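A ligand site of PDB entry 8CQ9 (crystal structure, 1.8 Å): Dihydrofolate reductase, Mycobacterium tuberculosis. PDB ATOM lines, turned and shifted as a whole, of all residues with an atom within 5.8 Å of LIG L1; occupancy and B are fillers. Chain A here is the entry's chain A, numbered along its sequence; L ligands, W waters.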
ATOM      1  N   ILE A   7      23.945 -13.484 -22.866  1.00  0.00           N
ATOM      2  CA  ILE A   7      24.101 -12.037 -22.849  1.00  0.00           C
ATOM      3  C   ILE A   7      23.552 -11.510 -21.518  1.00  0.00           C
ATOM      4  O   ILE A   7      22.433 -11.865 -21.118  1.00  0.00           O
ATOM      5  CB  ILE A   7      23.415 -11.406 -24.068  1.00  0.00           C
ATOM      6  CG1 ILE A   7      23.568  -9.884 -24.093  1.00  0.00           C
ATOM      7  CG2 ILE A   7      21.934 -11.837 -24.183  1.00  0.00           C
ATOM      8  CD1 ILE A   7      23.345  -9.283 -25.482  1.00  0.00           C
ATOM      9  N   TRP A   8      24.344 -10.694 -20.822  1.00  0.00           N
ATOM     10  CA  TRP A   8      23.904 -10.129 -19.547  1.00  0.00           C
ATOM     11  C   TRP A   8      24.652  -8.828 -19.289  1.00  0.00           C
ATOM     12  O   TRP A   8      25.701  -8.554 -19.867  1.00  0.00           O
ATOM     13  CB  TRP A   8      24.111 -11.101 -18.378  1.00  0.00           C
ATOM     14  CG  TRP A   8      25.516 -11.281 -17.836  1.00  0.00           C
ATOM     15  CD1 TRP A   8      26.200 -10.451 -16.985  1.00  0.00           C
ATOM     16  CD2 TRP A   8      26.374 -12.391 -18.091  1.00  0.00           C
ATOM     17  NE1 TRP A   8      27.450 -10.976 -16.707  1.00  0.00           N
ATOM     18  CE2 TRP A   8      27.576 -12.168 -17.373  1.00  0.00           C
ATOM     19  CE3 TRP A   8      26.251 -13.564 -18.851  1.00  0.00           C
ATOM     20  CZ2 TRP A   8      28.631 -13.074 -17.405  1.00  0.00           C
ATOM     21  CZ3 TRP A   8      27.302 -14.450 -18.881  1.00  0.00           C
ATOM     22  CH2 TRP A   8      28.479 -14.201 -18.169  1.00  0.00           C
ATOM     23  N   ALA A   9      24.082  -8.028 -18.392  1.00  0.00           N
ATOM     24  CA  ALA A   9      24.738  -6.848 -17.820  1.00  0.00           C
ATOM     25  C   ALA A   9      24.894  -7.073 -16.324  1.00  0.00           C
ATOM     26  O   ALA A   9      23.988  -7.601 -15.676  1.00  0.00           O
ATOM     27  CB  ALA A   9      23.893  -5.594 -18.074  1.00  0.00           C
ATOM     28  N   ILE A  22      16.062  -5.107 -12.090  1.00  0.00           N
ATOM     29  CA  ILE A  22      17.462  -4.711 -12.316  1.00  0.00           C
ATOM     30  C   ILE A  22      17.663  -3.293 -11.786  1.00  0.00           C
ATOM     31  O   ILE A  22      16.857  -2.406 -12.092  1.00  0.00           O
ATOM     32  CB  ILE A  22      17.836  -4.828 -13.801  1.00  0.00           C
ATOM     33  CG1 ILE A  22      17.602  -6.242 -14.333  1.00  0.00           C
ATOM     34  CG2 ILE A  22      19.298  -4.420 -14.020  1.00  0.00           C
ATOM     35  CD1 ILE A  22      17.682  -6.336 -15.842  1.00  0.00           C
ATOM     36  N   ASP A  29      22.875   0.005 -23.762  1.00  0.00           N
ATOM     37  CA  ASP A  29      23.039  -1.441 -23.629  1.00  0.00           C
ATOM     38  C   ASP A  29      21.797  -2.175 -24.128  1.00  0.00           C
ATOM     39  O   ASP A  29      21.911  -3.241 -24.743  1.00  0.00           O
ATOM     40  CB  ASP A  29      23.313  -1.801 -22.173  1.00  0.00           C
ATOM     41  CG  ASP A  29      23.882  -3.193 -22.043  1.00  0.00           C
ATOM     42  OD1 ASP A  29      24.786  -3.522 -22.840  1.00  0.00           O
ATOM     43  OD2 ASP A  29      23.453  -3.923 -21.149  1.00  0.00           O
ATOM     44  N   GLN A  30      20.614  -1.626 -23.864  1.00  0.00           N
ATOM     45  CA  GLN A  30      19.404  -2.237 -24.404  1.00  0.00           C
ATOM     46  C   GLN A  30      19.450  -2.297 -25.921  1.00  0.00           C
ATOM     47  O   GLN A  30      19.039  -3.299 -26.530  1.00  0.00           O
ATOM     48  CB  GLN A  30      18.184  -1.458 -23.947  1.00  0.00           C
ATOM     49  CG  GLN A  30      18.137  -1.306 -22.435  1.00  0.00           C
ATOM     50  CD  GLN A  30      16.781  -0.840 -22.007  1.00  0.00           C
ATOM     51  OE1 GLN A  30      16.133  -0.096 -22.724  1.00  0.00           O
ATOM     52  NE2 GLN A  30      16.347  -1.270 -20.827  1.00  0.00           N
ATOM     53  N   PHE A  33      21.747  -5.090 -26.785  1.00  0.00           N
ATOM     54  CA  PHE A  33      21.011  -6.332 -26.562  1.00  0.00           C
ATOM     55  C   PHE A  33      20.061  -6.623 -27.726  1.00  0.00           C
ATOM     56  O   PHE A  33      20.023  -7.752 -28.230  1.00  0.00           O
ATOM     57  CB  PHE A  33      20.270  -6.255 -25.233  1.00  0.00           C
ATOM     58  CG  PHE A  33      19.274  -7.376 -25.022  1.00  0.00           C
ATOM     59  CD1 PHE A  33      19.659  -8.556 -24.402  1.00  0.00           C
ATOM     60  CD2 PHE A  33      17.948  -7.223 -25.437  1.00  0.00           C
ATOM     61  CE1 PHE A  33      18.747  -9.596 -24.207  1.00  0.00           C
ATOM     62  CE2 PHE A  33      17.016  -8.256 -25.249  1.00  0.00           C
ATOM     63  CZ  PHE A  33      17.435  -9.450 -24.627  1.00  0.00           C
ATOM     64  N   MET A  44      14.845 -17.658 -21.722  1.00  0.00           N
ATOM     65  CA  MET A  44      14.806 -16.937 -20.453  1.00  0.00           C
ATOM     66  C   MET A  44      14.117 -17.797 -19.409  1.00  0.00           C
ATOM     67  O   MET A  44      13.206 -18.573 -19.717  1.00  0.00           O
ATOM     68  CB  MET A  44      14.111 -15.591 -20.702  1.00  0.00           C
ATOM     69  CG  MET A  44      12.617 -15.711 -20.875  1.00  0.00           C
ATOM     70  SD  MET A  44      11.828 -14.125 -21.153  1.00  0.00           S
ATOM     71  CE  MET A  44      11.889 -14.187 -22.941  1.00  0.00           C
ATOM     72  N   THR A  48      12.434 -14.256 -15.186  1.00  0.00           N
ATOM     73  CA  THR A  48      12.771 -13.163 -16.107  1.00  0.00           C
ATOM     74  C   THR A  48      11.611 -12.834 -17.036  1.00  0.00           C
ATOM     75  O   THR A  48      11.322 -11.659 -17.285  1.00  0.00           O
ATOM     76  CB  THR A  48      14.035 -13.502 -16.883  1.00  0.00           C
ATOM     77  OG1 THR A  48      15.143 -13.584 -15.976  1.00  0.00           O
ATOM     78  CG2 THR A  48      14.330 -12.467 -17.933  1.00  0.00           C
ATOM     79  N   SER A  51       9.357 -10.616 -15.221  1.00  0.00           N
ATOM     80  CA  SER A  51       9.895  -9.253 -15.109  1.00  0.00           C
ATOM     81  C   SER A  51       9.611  -8.404 -16.334  1.00  0.00           C
ATOM     82  O   SER A  51       9.777  -7.173 -16.286  1.00  0.00           O
ATOM     83  CB  SER A  51      11.406  -9.310 -14.862  1.00  0.00           C
ATOM     84  OG  SER A  51      12.139  -9.439 -16.084  1.00  0.00           O
ATOM     85  N   LEU A  52       9.204  -9.028 -17.446  1.00  0.00           N
ATOM     86  CA  LEU A  52       8.860  -8.256 -18.634  1.00  0.00           C
ATOM     87  C   LEU A  52       7.413  -7.777 -18.542  1.00  0.00           C
ATOM     88  O   LEU A  52       6.523  -8.585 -18.261  1.00  0.00           O
ATOM     89  CB  LEU A  52       9.012  -9.099 -19.887  1.00  0.00           C
ATOM     90  CG  LEU A  52      10.461  -9.394 -20.287  1.00  0.00           C
ATOM     91  CD1 LEU A  52      10.458 -10.493 -21.356  1.00  0.00           C
ATOM     92  CD2 LEU A  52      11.191  -8.139 -20.764  1.00  0.00           C
ATOM     93  N   LEU A  59       9.280 -10.400 -26.893  1.00  0.00           N
ATOM     94  CA  LEU A  59      10.196  -9.442 -27.500  1.00  0.00           C
ATOM     95  C   LEU A  59      10.155  -9.632 -29.024  1.00  0.00           C
ATOM     96  O   LEU A  59      10.319 -10.762 -29.507  1.00  0.00           O
ATOM     97  CB  LEU A  59      11.612  -9.630 -26.954  1.00  0.00           C
ATOM     98  CG  LEU A  59      11.861  -9.476 -25.457  1.00  0.00           C
ATOM     99  CD1 LEU A  59      13.359  -9.355 -25.172  1.00  0.00           C
ATOM    100  CD2 LEU A  59      11.083  -8.315 -24.814  1.00  0.00           C
ATOM    101  N   VAL A  95      20.780 -16.860 -24.605  1.00  0.00           N
ATOM    102  CA  VAL A  95      20.213 -17.046 -23.271  1.00  0.00           C
ATOM    103  C   VAL A  95      20.245 -15.688 -22.594  1.00  0.00           C
ATOM    104  O   VAL A  95      21.308 -15.092 -22.431  1.00  0.00           O
ATOM    105  CB  VAL A  95      21.005 -18.096 -22.471  1.00  0.00           C
ATOM    106  CG1 VAL A  95      20.488 -18.178 -21.040  1.00  0.00           C
ATOM    107  CG2 VAL A  95      20.910 -19.456 -23.154  1.00  0.00           C
ATOM    108  N   ILE A  96      19.068 -15.155 -22.264  1.00  0.00           N
ATOM    109  CA  ILE A  96      18.995 -13.754 -21.835  1.00  0.00           C
ATOM    110  C   ILE A  96      18.682 -13.625 -20.343  1.00  0.00           C
ATOM    111  O   ILE A  96      18.319 -12.554 -19.891  1.00  0.00           O
ATOM    112  CB  ILE A  96      17.992 -12.976 -22.710  1.00  0.00           C
ATOM    113  CG1 ILE A  96      16.562 -13.469 -22.505  1.00  0.00           C
ATOM    114  CG2 ILE A  96      18.346 -13.162 -24.173  1.00  0.00           C
ATOM    115  CD1 ILE A  96      15.520 -12.441 -22.975  1.00  0.00           C
ATOM    116  N   GLY A  97      18.824 -14.695 -19.574  1.00  0.00           N
ATOM    117  CA  GLY A  97      18.720 -14.631 -18.125  1.00  0.00           C
ATOM    118  C   GLY A  97      17.603 -15.513 -17.569  1.00  0.00           C
ATOM    119  O   GLY A  97      16.844 -16.144 -18.304  1.00  0.00           O
ATOM    120  N   TYR A 102      21.362 -18.764 -16.690  1.00  0.00           N
ATOM    121  CA  TYR A 102      22.749 -18.584 -17.149  1.00  0.00           C
ATOM    122  C   TYR A 102      23.610 -19.743 -16.672  1.00  0.00           C
ATOM    123  O   TYR A 102      24.376 -20.330 -17.444  1.00  0.00           O
ATOM    124  CB  TYR A 102      23.343 -17.268 -16.635  1.00  0.00           C
ATOM    125  CG  TYR A 102      22.774 -16.015 -17.245  1.00  0.00           C
ATOM    126  CD1 TYR A 102      22.506 -14.928 -16.428  1.00  0.00           C
ATOM    127  CD2 TYR A 102      22.580 -15.892 -18.622  1.00  0.00           C
ATOM    128  CE1 TYR A 102      22.009 -13.761 -16.945  1.00  0.00           C
ATOM    129  CE2 TYR A 102      22.084 -14.713 -19.147  1.00  0.00           C
ATOM    130  CZ  TYR A 102      21.788 -13.658 -18.282  1.00  0.00           C
ATOM    131  OH  TYR A 102      21.302 -12.472 -18.758  1.00  0.00           O
ATOM    132  N   GLU A 113      28.278 -12.292 -24.048  1.00  0.00           N
ATOM    133  CA  GLU A 113      28.353 -10.847 -24.288  1.00  0.00           C
ATOM    134  C   GLU A 113      27.999 -10.186 -22.968  1.00  0.00           C
ATOM    135  O   GLU A 113      26.833 -10.191 -22.568  1.00  0.00           O
ATOM    136  CB  GLU A 113      27.399 -10.425 -25.408  1.00  0.00           C
ATOM    137  CG  GLU A 113      27.800 -10.956 -26.804  1.00  0.00           C
ATOM    138  CD  GLU A 113      29.008 -10.206 -27.389  1.00  0.00           C
ATOM    139  OE1 GLU A 113      29.021  -8.960 -27.306  1.00  0.00           O
ATOM    140  OE2 GLU A 113      29.935 -10.864 -27.929  1.00  0.00           O
ATOM    141  N   THR A 115      27.999  -6.978 -20.378  1.00  0.00           N
ATOM    142  CA  THR A 115      28.133  -5.547 -20.141  1.00  0.00           C
ATOM    143  C   THR A 115      28.454  -5.345 -18.670  1.00  0.00           C
ATOM    144  O   THR A 115      27.715  -5.829 -17.798  1.00  0.00           O
ATOM    145  CB  THR A 115      26.862  -4.782 -20.505  1.00  0.00           C
ATOM    146  OG1 THR A 115      26.591  -4.971 -21.896  1.00  0.00           O
ATOM    147  CG2 THR A 115      27.041  -3.273 -20.223  1.00  0.00           C
HETATM  148  C1  LIG L   1      14.390  -9.625 -20.672  1.00  0.00           C
HETATM  149  C2  LIG L   1      18.655  -5.396 -20.188  1.00  0.00           C
HETATM  150  C3  LIG L   1      21.808  -7.111 -21.330  1.00  0.00           C
HETATM  151  C4  LIG L   1      20.305  -8.800 -21.004  1.00  0.00           C
HETATM  152  C5  LIG L   1      19.315  -7.864 -20.617  1.00  0.00           C
HETATM  153  C6  LIG L   1      17.868  -8.205 -20.214  1.00  0.00           C
HETATM  154  C7  LIG L   1      17.143  -9.094 -20.860  1.00  0.00           C
HETATM  155  C8  LIG L   1      15.706  -9.296 -20.382  1.00  0.00           C
HETATM  156  C9  LIG L   1      14.740  -9.204 -19.391  1.00  0.00           C
HETATM  157  C10 LIG L   1      19.677  -6.507 -20.604  1.00  0.00           C
HETATM  158  N1  LIG L   1      23.150  -6.703 -21.700  1.00  0.00           N
HETATM  159  N2  LIG L   1      21.518  -8.401 -21.354  1.00  0.00           N
HETATM  160  N3  LIG L   1      20.063 -10.218 -21.086  1.00  0.00           N
HETATM  161  N4  LIG L   1      20.910  -6.184 -20.972  1.00  0.00           N
HETATM  162  P1  LG2 L   2      15.481 -17.023 -13.740  1.00  0.00           P
HETATM  163  O1  LG2 L   2      15.092 -15.853 -14.586  1.00  0.00           O
HETATM  164  O2  LG2 L   2      16.790 -17.726 -13.934  1.00  0.00           O
HETATM  165  O3  LG2 L   2      14.206 -18.045 -13.776  1.00  0.00           O
HETATM  166  C1  LG2 L   2      14.348 -19.037 -12.750  1.00  0.00           C
HETATM  167  C2  LG2 L   2      13.177 -20.039 -13.091  1.00  0.00           C
HETATM  168  O4  LG2 L   2      13.444 -20.685 -14.324  1.00  0.00           O
HETATM  169  C3  LG2 L   2      12.859 -21.119 -12.049  1.00  0.00           C
HETATM  170  O5  LG2 L   2      12.019 -20.582 -11.030  1.00  0.00           O
HETATM  171  C4  LG2 L   2      12.029 -22.088 -12.944  1.00  0.00           C
HETATM  172  O6  LG2 L   2      10.852 -21.592 -13.296  1.00  0.00           O
HETATM  173  C5  LG2 L   2      12.902 -22.027 -14.246  1.00  0.00           C
HETATM  174  N1  LG2 L   2      14.000 -22.949 -14.219  1.00  0.00           N
HETATM  175  C6  LG2 L   2      15.261 -22.792 -13.653  1.00  0.00           C
HETATM  176  N2  LG2 L   2      16.046 -23.886 -13.805  1.00  0.00           N
HETATM  177  C7  LG2 L   2      15.240 -24.789 -14.489  1.00  0.00           C
HETATM  178  C8  LG2 L   2      15.460 -26.114 -14.951  1.00  0.00           C
HETATM  179  N3  LG2 L   2      16.655 -26.756 -14.752  1.00  0.00           N
HETATM  180  N4  LG2 L   2      14.481 -26.797 -15.625  1.00  0.00           N
HETATM  181  C9  LG2 L   2      13.295 -26.105 -15.789  1.00  0.00           C
HETATM  182  N5  LG2 L   2      12.952 -24.858 -15.417  1.00  0.00           N
HETATM  183  C10 LG2 L   2      13.956 -24.209 -14.760  1.00  0.00           C
HETATM  184  O7  LG2 L   2      15.373 -16.481 -12.137  1.00  0.00           O
HETATM  185  P2  LG2 L   2      16.590 -15.724 -11.401  1.00  0.00           P
HETATM  186  O8  LG2 L   2      15.974 -15.255 -10.143  1.00  0.00           O
HETATM  187  O9  LG2 L   2      17.884 -16.487 -11.326  1.00  0.00           O
HETATM  188  O10 LG2 L   2      16.948 -14.339 -12.325  1.00  0.00           O
HETATM  189  C11 LG2 L   2      15.920 -13.375 -12.204  1.00  0.00           C
HETATM  190  C12 LG2 L   2      16.622 -12.023 -11.935  1.00  0.00           C
HETATM  191  O11 LG2 L   2      17.615 -11.798 -12.977  1.00  0.00           O
HETATM  192  C13 LG2 L   2      15.610 -10.816 -11.960  1.00  0.00           C
HETATM  193  O12 LG2 L   2      16.047  -9.860 -11.028  1.00  0.00           O
HETATM  194  C14 LG2 L   2      15.851 -10.290 -13.383  1.00  0.00           C
HETATM  195  O13 LG2 L   2      15.551  -8.935 -13.503  1.00  0.00           O
HETATM  196  C15 LG2 L   2      17.394 -10.491 -13.492  1.00  0.00           C
HETATM  197  N6  LG2 L   2      17.917 -10.452 -14.894  1.00  0.00           N
HETATM  198  C16 LG2 L   2      19.019  -9.651 -15.174  1.00  0.00           C
HETATM  199  C17 LG2 L   2      19.560  -9.634 -16.417  1.00  0.00           C
HETATM  200  C18 LG2 L   2      20.716  -8.845 -16.664  1.00  0.00           C
HETATM  201  O14 LG2 L   2      21.394  -8.942 -17.705  1.00  0.00           O
HETATM  202  N7  LG2 L   2      21.131  -7.979 -15.703  1.00  0.00           N
HETATM  203  C19 LG2 L   2      18.994 -10.413 -17.539  1.00  0.00           C
HETATM  204  C20 LG2 L   2      17.854 -11.254 -17.140  1.00  0.00           C
HETATM  205  C21 LG2 L   2      17.358 -11.272 -15.898  1.00  0.00           C
HETATM  206  P3  LG2 L   2       9.456 -22.205 -12.401  1.00  0.00           P
HETATM  207  O15 LG2 L   2       8.381 -21.579 -13.237  1.00  0.00           O
HETATM  208  O16 LG2 L   2       9.627 -23.720 -12.499  1.00  0.00           O
HETATM  209  O17 LG2 L   2       9.699 -21.589 -11.030  1.00  0.00           O
HETATM  210  O   HOH W   1      24.394  -5.630 -24.709  1.00  0.00           O
HETATM  211  O   HOH W   2      25.679  -7.454 -22.801  1.00  0.00           O
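The side-chain carboxylate (OD1) of Asp 29 lies within hydrogen-bond range of the side-chain hydroxyl (OG1) of Thr 115 (2.5 Å).
The backbone carbonyl oxygen (O) of Ile 7 lies within hydrogen-bond range of the side-chain hydroxyl (OH) of Tyr 102, 2.7 Å away.
The backbone carbonyl oxygen (O) of Val 95 sits at hydrogen-bond distance from the backbone NH (N) of Ile 7.
OH of Tyr 102 is in hydrogen-bond range of O of Ile 96 (3.2 Å).
N of Thr 115 sits at hydrogen-bond distance from O of Trp 8 (2.8 Å).
The backbone NH of Trp 8 lies within hydrogen-bond range of the backbone carbonyl oxygen of Glu 113 (3.1 Å).
The side-chain hydroxyl (OH) of Tyr 102 sits close to the backbone NH (N) of Gly 97.
O of Thr 48 is in hydrogen-bond range of OG of Ser 51 (2.7 Å).
Water W2 lies within hydrogen-bond range of the side-chain hydroxyl (OG1) of Thr 115 (2.8 Å), a nitrogen (N1) of LIG L1 (2.9 Å), the backbone carbonyl oxygen (O) of Glu 113 (3.0 Å) and the backbone carbonyl oxygen (O) of Trp 8 (3.1 Å).
Water W1 lies within hydrogen-bond range of the side-chain carboxylate of Asp 29, the backbone NH of Phe 33 and a nitrogen (N1) of LIG L1.
CA of Trp 8 touches N2 of LIG L1, at 3.5 Å.
N of Ala 9 touches N1 of LIG L1 (3.7 Å).
Phe 33 touches LIG L1.
Thr 48 touches LIG L1.
Leu 52 touches LIG L1.
Thr 115 touches LIG L1 (OG1 to N1, 3.9 Å).
OD2 of Asp 29 sits at hydrogen-bond distance from N1 of LIG L1 (2.9 Å).
A nitrogen (N3) of LIG L1 lies within hydrogen-bond range of the backbone carbonyl oxygen (O) of Ile 7.
The backbone carbonyl oxygen of Ile 96 sits at hydrogen-bond distance from a nitrogen (N3) of LIG L1 (3.2 Å).
The side-chain hydroxyl of Tyr 102 sits at hydrogen-bond distance from a nitrogen (N3) of LIG L1, at 3.5 Å.
The backbone NH (N) of Thr 48 is in hydrogen-bond range of an oxygen (O1) of LG2 L2 (3.2 Å).
O1 of LG2 L2 sits at hydrogen-bond distance from OG1 of Thr 48, 2.7 Å away.
An oxygen (O14) of LG2 L2 sits at hydrogen-bond distance from the backbone NH (N) of Ala 9 (2.9 Å).
The backbone carbonyl oxygen (O) of Ala 9 lies within hydrogen-bond range of a nitrogen (N7) of LG2 L2 (2.9 Å).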
